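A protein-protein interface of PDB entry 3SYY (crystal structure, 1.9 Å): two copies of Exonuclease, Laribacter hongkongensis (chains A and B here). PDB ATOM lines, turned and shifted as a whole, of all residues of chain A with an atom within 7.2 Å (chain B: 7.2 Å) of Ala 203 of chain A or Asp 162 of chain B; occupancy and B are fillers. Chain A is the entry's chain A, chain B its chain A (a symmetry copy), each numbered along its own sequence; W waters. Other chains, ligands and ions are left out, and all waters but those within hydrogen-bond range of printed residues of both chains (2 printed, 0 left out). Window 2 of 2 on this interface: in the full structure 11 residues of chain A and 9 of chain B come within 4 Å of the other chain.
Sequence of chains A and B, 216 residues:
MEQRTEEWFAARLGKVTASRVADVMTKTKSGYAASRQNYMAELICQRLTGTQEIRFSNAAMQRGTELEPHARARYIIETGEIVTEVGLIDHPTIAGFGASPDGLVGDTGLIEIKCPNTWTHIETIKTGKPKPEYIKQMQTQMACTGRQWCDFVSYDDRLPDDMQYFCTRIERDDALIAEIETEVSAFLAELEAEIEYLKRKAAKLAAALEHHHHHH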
ATOM      1  N   TYR A 197     -22.229  -4.367   0.520  1.00  0.00           N
ATOM      2  CA  TYR A 197     -21.594  -5.669   0.575  1.00  0.00           C
ATOM      3  C   TYR A 197     -22.209  -6.614   1.561  1.00  0.00           C
ATOM      4  O   TYR A 197     -22.519  -7.777   1.205  1.00  0.00           O
ATOM      5  CB  TYR A 197     -20.133  -5.482   0.868  1.00  0.00           C
ATOM      6  CG  TYR A 197     -19.189  -6.600   0.541  1.00  0.00           C
ATOM      7  CD1 TYR A 197     -19.008  -7.052  -0.798  1.00  0.00           C
ATOM      8  CD2 TYR A 197     -18.383  -7.149   1.543  1.00  0.00           C
ATOM      9  CE1 TYR A 197     -18.060  -8.023  -1.088  1.00  0.00           C
ATOM     10  CE2 TYR A 197     -17.471  -8.159   1.266  1.00  0.00           C
ATOM     11  CZ  TYR A 197     -17.315  -8.587  -0.056  1.00  0.00           C
ATOM     12  OH  TYR A 197     -16.349  -9.509  -0.322  1.00  0.00           O
ATOM     13  N   LEU A 198     -22.387  -6.156   2.806  1.00  0.00           N
ATOM     14  CA  LEU A 198     -23.040  -6.974   3.820  1.00  0.00           C
ATOM     15  C   LEU A 198     -24.451  -7.369   3.395  1.00  0.00           C
ATOM     16  O   LEU A 198     -24.890  -8.534   3.580  1.00  0.00           O
ATOM     17  CB  LEU A 198     -23.148  -6.225   5.139  1.00  0.00           C
ATOM     18  CG  LEU A 198     -22.000  -6.249   6.156  1.00  0.00           C
ATOM     19  CD1 LEU A 198     -20.797  -7.154   5.862  1.00  0.00           C
ATOM     20  CD2 LEU A 198     -21.602  -4.808   6.654  1.00  0.00           C
ATOM     21  N   LYS A 199     -25.173  -6.398   2.869  1.00  0.00           N
ATOM     22  CA  LYS A 199     -26.564  -6.629   2.478  1.00  0.00           C
ATOM     23  C   LYS A 199     -26.699  -7.670   1.322  1.00  0.00           C
ATOM     24  O   LYS A 199     -27.591  -8.551   1.370  1.00  0.00           O
ATOM     25  CB  LYS A 199     -27.255  -5.299   2.122  1.00  0.00           C
ATOM     26  CG  LYS A 199     -27.853  -4.537   3.334  1.00  0.00           C
ATOM     27  CD  LYS A 199     -28.488  -3.252   2.828  1.00  0.00           C
ATOM     28  CE  LYS A 199     -29.056  -2.459   3.949  1.00  0.00           C
ATOM     29  NZ  LYS A 199     -29.264  -1.045   3.462  1.00  0.00           N
ATOM     30  N   ARG A 200     -25.850  -7.522   0.305  1.00  0.00           N
ATOM     31  CA  ARG A 200     -25.830  -8.429  -0.866  1.00  0.00           C
ATOM     32  C   ARG A 200     -25.505  -9.849  -0.439  1.00  0.00           C
ATOM     33  O   ARG A 200     -26.211 -10.796  -0.825  1.00  0.00           O
ATOM     34  CB  ARG A 200     -24.843  -7.921  -1.904  1.00  0.00           C
ATOM     35  CG  ARG A 200     -25.434  -6.776  -2.728  1.00  0.00           C
ATOM     36  CD  ARG A 200     -24.518  -6.379  -3.827  1.00  0.00           C
ATOM     37  NE  ARG A 200     -25.083  -5.321  -4.664  1.00  0.00           N
ATOM     38  CZ  ARG A 200     -25.920  -5.516  -5.685  1.00  0.00           C
ATOM     39  NH1 ARG A 200     -26.344  -6.734  -6.015  1.00  0.00           N
ATOM     40  NH2 ARG A 200     -26.336  -4.473  -6.381  1.00  0.00           N
ATOM     41  N   LYS A 201     -24.509  -9.988   0.445  1.00  0.00           N
ATOM     42  CA  LYS A 201     -24.181 -11.292   1.023  1.00  0.00           C
ATOM     43  C   LYS A 201     -25.304 -11.905   1.785  1.00  0.00           C
ATOM     44  O   LYS A 201     -25.578 -13.084   1.566  1.00  0.00           O
ATOM     45  CB  LYS A 201     -22.958 -11.228   1.933  1.00  0.00           C
ATOM     46  CG  LYS A 201     -21.696 -11.161   1.176  1.00  0.00           C
ATOM     47  CD  LYS A 201     -20.512 -11.051   2.133  1.00  0.00           C
ATOM     48  CE  LYS A 201     -19.264 -11.513   1.414  1.00  0.00           C
ATOM     49  NZ  LYS A 201     -18.019 -11.338   2.243  1.00  0.00           N
ATOM     50  N   ALA A 202     -25.945 -11.141   2.685  1.00  0.00           N
ATOM     51  CA  ALA A 202     -27.048 -11.675   3.466  1.00  0.00           C
ATOM     52  C   ALA A 202     -28.233 -12.056   2.565  1.00  0.00           C
ATOM     53  O   ALA A 202     -28.883 -13.095   2.789  1.00  0.00           O
ATOM     54  CB  ALA A 202     -27.483 -10.708   4.563  1.00  0.00           C
ATOM     55  N   ALA A 203     -28.507 -11.208   1.569  1.00  0.00           N
ATOM     56  CA  ALA A 203     -29.637 -11.419   0.656  1.00  0.00           C
ATOM     57  C   ALA A 203     -29.431 -12.704  -0.201  1.00  0.00           C
ATOM     58  O   ALA A 203     -30.343 -13.542  -0.336  1.00  0.00           O
ATOM     59  CB  ALA A 203     -29.874 -10.167  -0.213  1.00  0.00           C
ATOM     60  N   LYS A 204     -28.237 -12.857  -0.757  1.00  0.00           N
ATOM     61  CA  LYS A 204     -27.900 -14.040  -1.509  1.00  0.00           C
ATOM     62  C   LYS A 204     -28.063 -15.277  -0.634  1.00  0.00           C
ATOM     63  O   LYS A 204     -28.713 -16.261  -1.037  1.00  0.00           O
ATOM     64  CB  LYS A 204     -26.477 -13.941  -2.027  1.00  0.00           C
ATOM     65  CG  LYS A 204     -26.165 -14.887  -3.160  1.00  0.00           C
ATOM     66  CD  LYS A 204     -24.870 -15.619  -2.910  1.00  0.00           C
ATOM     67  CE  LYS A 204     -23.969 -15.612  -4.125  1.00  0.00           C
ATOM     68  NZ  LYS A 204     -23.881 -14.264  -4.754  1.00  0.00           N
ATOM     69  N   LEU A 205     -27.495 -15.212   0.578  1.00  0.00           N
ATOM     70  CA  LEU A 205     -27.600 -16.301   1.554  1.00  0.00           C
ATOM     71  C   LEU A 205     -29.027 -16.710   1.876  1.00  0.00           C
ATOM     72  O   LEU A 205     -29.316 -17.899   1.985  1.00  0.00           O
ATOM     73  CB  LEU A 205     -26.849 -15.938   2.850  1.00  0.00           C
ATOM     74  CG  LEU A 205     -26.038 -16.994   3.595  1.00  0.00           C
ATOM     75  CD1 LEU A 205     -26.871 -17.570   4.732  1.00  0.00           C
ATOM     76  CD2 LEU A 205     -25.543 -18.088   2.637  1.00  0.00           C
ATOM     77  N   ALA A 206     -29.921 -15.741   2.038  1.00  0.00           N
ATOM     78  CA  ALA A 206     -31.295 -16.039   2.429  1.00  0.00           C
ATOM     79  C   ALA A 206     -32.158 -16.593   1.273  1.00  0.00           C
ATOM     80  O   ALA A 206     -31.798 -16.454   0.097  1.00  0.00           O
ATOM     81  CB  ALA A 206     -31.955 -14.799   3.057  1.00  0.00           C
ATOM     82  N   ARG B  74     -35.121 -18.636  18.427  1.00  0.00           N
ATOM     83  CA  ARG B  74     -34.752 -18.516  17.024  1.00  0.00           C
ATOM     84  C   ARG B  74     -33.986 -19.735  16.508  1.00  0.00           C
ATOM     85  O   ARG B  74     -34.183 -20.179  15.348  1.00  0.00           O
ATOM     86  CB  ARG B  74     -33.952 -17.230  16.756  1.00  0.00           C
ATOM     87  CG  ARG B  74     -33.558 -17.023  15.282  1.00  0.00           C
ATOM     88  CD  ARG B  74     -34.814 -16.686  14.362  1.00  0.00           C
ATOM     89  NE  ARG B  74     -34.317 -16.151  13.091  1.00  0.00           N
ATOM     90  CZ  ARG B  74     -34.132 -14.855  12.800  1.00  0.00           C
ATOM     91  NH1 ARG B  74     -34.485 -13.890  13.646  1.00  0.00           N
ATOM     92  NH2 ARG B  74     -33.619 -14.512  11.628  1.00  0.00           N
ATOM     93  N   ILE B 125     -20.338 -12.801  11.487  1.00  0.00           N
ATOM     94  CA  ILE B 125     -20.877 -13.139  10.156  1.00  0.00           C
ATOM     95  C   ILE B 125     -19.792 -13.059   9.081  1.00  0.00           C
ATOM     96  O   ILE B 125     -19.675 -13.980   8.272  1.00  0.00           O
ATOM     97  CB  ILE B 125     -22.093 -12.316   9.823  1.00  0.00           C
ATOM     98  CG1 ILE B 125     -23.221 -12.745  10.771  1.00  0.00           C
ATOM     99  CG2 ILE B 125     -22.485 -12.436   8.295  1.00  0.00           C
ATOM    100  CD1 ILE B 125     -24.436 -11.865  10.667  1.00  0.00           C
ATOM    101  N   LEU B 159     -30.712  -5.894  13.960  1.00  0.00           N
ATOM    102  CA  LEU B 159     -30.298  -5.895  12.570  1.00  0.00           C
ATOM    103  C   LEU B 159     -31.476  -6.272  11.657  1.00  0.00           C
ATOM    104  O   LEU B 159     -32.465  -6.760  12.147  1.00  0.00           O
ATOM    105  CB  LEU B 159     -29.156  -6.890  12.397  1.00  0.00           C
ATOM    106  CG  LEU B 159     -27.819  -6.340  12.929  1.00  0.00           C
ATOM    107  CD1 LEU B 159     -26.807  -7.397  12.971  1.00  0.00           C
ATOM    108  CD2 LEU B 159     -27.300  -5.213  12.017  1.00  0.00           C
ATOM    109  N   PRO B 160     -31.351  -6.065  10.327  1.00  0.00           N
ATOM    110  CA  PRO B 160     -32.380  -6.591   9.393  1.00  0.00           C
ATOM    111  C   PRO B 160     -32.516  -8.110   9.582  1.00  0.00           C
ATOM    112  O   PRO B 160     -31.549  -8.761   9.990  1.00  0.00           O
ATOM    113  CB  PRO B 160     -31.738  -6.344   8.026  1.00  0.00           C
ATOM    114  CG  PRO B 160     -30.914  -5.096   8.250  1.00  0.00           C
ATOM    115  CD  PRO B 160     -30.257  -5.421   9.597  1.00  0.00           C
ATOM    116  N   ASP B 161     -33.687  -8.658   9.237  1.00  0.00           N
ATOM    117  CA  ASP B 161     -33.972 -10.070   9.459  1.00  0.00           C
ATOM    118  C   ASP B 161     -32.887 -11.002   8.938  1.00  0.00           C
ATOM    119  O   ASP B 161     -32.503 -11.936   9.650  1.00  0.00           O
ATOM    120  CB  ASP B 161     -35.353 -10.505   8.912  1.00  0.00           C
ATOM    121  CG  ASP B 161     -35.619 -12.004   9.191  1.00  0.00           C
ATOM    122  OD1 ASP B 161     -35.841 -12.389  10.379  1.00  0.00           O
ATOM    123  OD2 ASP B 161     -35.536 -12.802   8.231  1.00  0.00           O
ATOM    124  N   ASP B 162     -32.361 -10.735   7.736  1.00  0.00           N
ATOM    125  CA  ASP B 162     -31.442 -11.688   7.143  1.00  0.00           C
ATOM    126  C   ASP B 162     -30.020 -11.557   7.733  1.00  0.00           C
ATOM    127  O   ASP B 162     -29.120 -12.184   7.232  1.00  0.00           O
ATOM    128  CB  ASP B 162     -31.408 -11.563   5.595  1.00  0.00           C
ATOM    129  CG  ASP B 162     -30.988 -10.163   5.120  1.00  0.00           C
ATOM    130  OD1 ASP B 162     -31.034  -9.909   3.874  1.00  0.00           O
ATOM    131  OD2 ASP B 162     -30.608  -9.292   5.976  1.00  0.00           O
ATOM    132  N   MET B 163     -29.835 -10.708   8.753  1.00  0.00           N
ATOM    133  CA  MET B 163     -28.528 -10.606   9.459  1.00  0.00           C
ATOM    134  C   MET B 163     -28.608 -10.884  10.960  1.00  0.00           C
ATOM    135  O   MET B 163     -27.596 -10.818  11.633  1.00  0.00           O
ATOM    136  CB  MET B 163     -27.943  -9.193   9.295  1.00  0.00           C
ATOM    137  CG  MET B 163     -27.554  -8.851   7.903  1.00  0.00           C
ATOM    138  SD  MET B 163     -26.809  -7.171   7.867  1.00  0.00           S
ATOM    139  CE  MET B 163     -26.671  -6.909   6.098  1.00  0.00           C
ATOM    140  N   GLN B 164     -29.792 -11.193  11.481  1.00  0.00           N
ATOM    141  CA  GLN B 164     -29.991 -11.306  12.917  1.00  0.00           C
ATOM    142  C   GLN B 164     -29.376 -12.595  13.482  1.00  0.00           C
ATOM    143  O   GLN B 164     -28.936 -12.611  14.654  1.00  0.00           O
ATOM    144  CB  GLN B 164     -31.456 -11.267  13.254  1.00  0.00           C
ATOM    145  CG  GLN B 164     -32.105  -9.893  13.001  1.00  0.00           C
ATOM    146  CD  GLN B 164     -33.609  -9.883  13.206  1.00  0.00           C
ATOM    147  OE1 GLN B 164     -34.242  -8.801  13.220  1.00  0.00           O
ATOM    148  NE2 GLN B 164     -34.204 -11.048  13.324  1.00  0.00           N
ATOM    149  N   TYR B 165     -29.353 -13.657  12.656  1.00  0.00           N
ATOM    150  CA  TYR B 165     -29.080 -15.012  13.154  1.00  0.00           C
ATOM    151  C   TYR B 165     -27.904 -15.660  12.487  1.00  0.00           C
ATOM    152  O   TYR B 165     -27.820 -15.664  11.252  1.00  0.00           O
ATOM    153  CB  TYR B 165     -30.331 -15.879  13.000  1.00  0.00           C
ATOM    154  CG  TYR B 165     -30.102 -17.324  13.354  1.00  0.00           C
ATOM    155  CD1 TYR B 165     -30.164 -17.759  14.678  1.00  0.00           C
ATOM    156  CD2 TYR B 165     -29.861 -18.260  12.347  1.00  0.00           C
ATOM    157  CE1 TYR B 165     -29.979 -19.122  14.998  1.00  0.00           C
ATOM    158  CE2 TYR B 165     -29.691 -19.595  12.629  1.00  0.00           C
ATOM    159  CZ  TYR B 165     -29.760 -20.035  13.939  1.00  0.00           C
ATOM    160  OH  TYR B 165     -29.563 -21.381  14.142  1.00  0.00           O
HETATM  161  O   HOH W   1     -28.976 -14.176   5.298  1.00  0.00           O
HETATM  162  O   HOH W   2     -29.809  -8.035   2.686  1.00  0.00           O
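Among the printed residues, merely in contact across the chains: Ala 202 of chain A with Asp 162 of chain B (3.5 Å), Leu 198 of chain A with Met 163 of chain B (3.5 Å), Lys 199 of chain A with Met 163 of chain B (3.6 Å), Ala 203 of chain A with Asp 162 of chain B (3.7 Å) and Ala 202 of chain A with Met 163 of chain B (3.8 Å).
Hydrophobic or aromatic side chains of chain B that line the printed part of chain A: Met 163. Of the 10 printed residues of chain A, 4 touch a printed residue of chain B. Hydrophobic or aromatic side chains of chain A within 4 Å of the printed part of chain B: Leu 198 and Ala 202. Among the printed residues, no Asp or Glu carboxylate lies within 4 Å of a Lys or Arg side-chain nitrogen of the other chain.
Printed residues of chain B within 4 Å of Leu 198 of chain A: Met 163. Of the printed residues of chain B, Lys 199 of chain A touches Met 163. Of the printed residues of chain B, Ala 202 of chain A touches Asp 162 and Met 163. Arg 74 of chain B touches none of the printed residues of chain A. Leu 159 of chain B touches none of the printed residues of chain A. Of the printed residues of chain A, Asp 162 of chain B touches Ala 202 and Ala 203. Of the printed residues of chain A, Met 163 of chain B touches Leu 198 (3.5 Å), Lys 199 (3.6 Å) and Ala 202 (3.8 Å). The nearest residue of chain B that does not touch Ala 203 of chain A is Met 163 of chain B (6.5 Å). The nearest printed residue of chain A that does not touch Met 163 of chain B is Arg 200 of chain A (5.9 Å).
Water W2 lies within hydrogen-bond range of the side-chain carboxylate of Asp 162 of chain B and the backbone carbonyl oxygen of Lys 199 of chain A. Water W1 bridges O of Ala 202 of chain A (2.7 Å) and O of Asp 162 of chain B (2.8 Å).
No position is printed for both chains. Of the 5 pairs that touch across the chains among the printed residues, none has its exchanged pair printed and touching as well.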
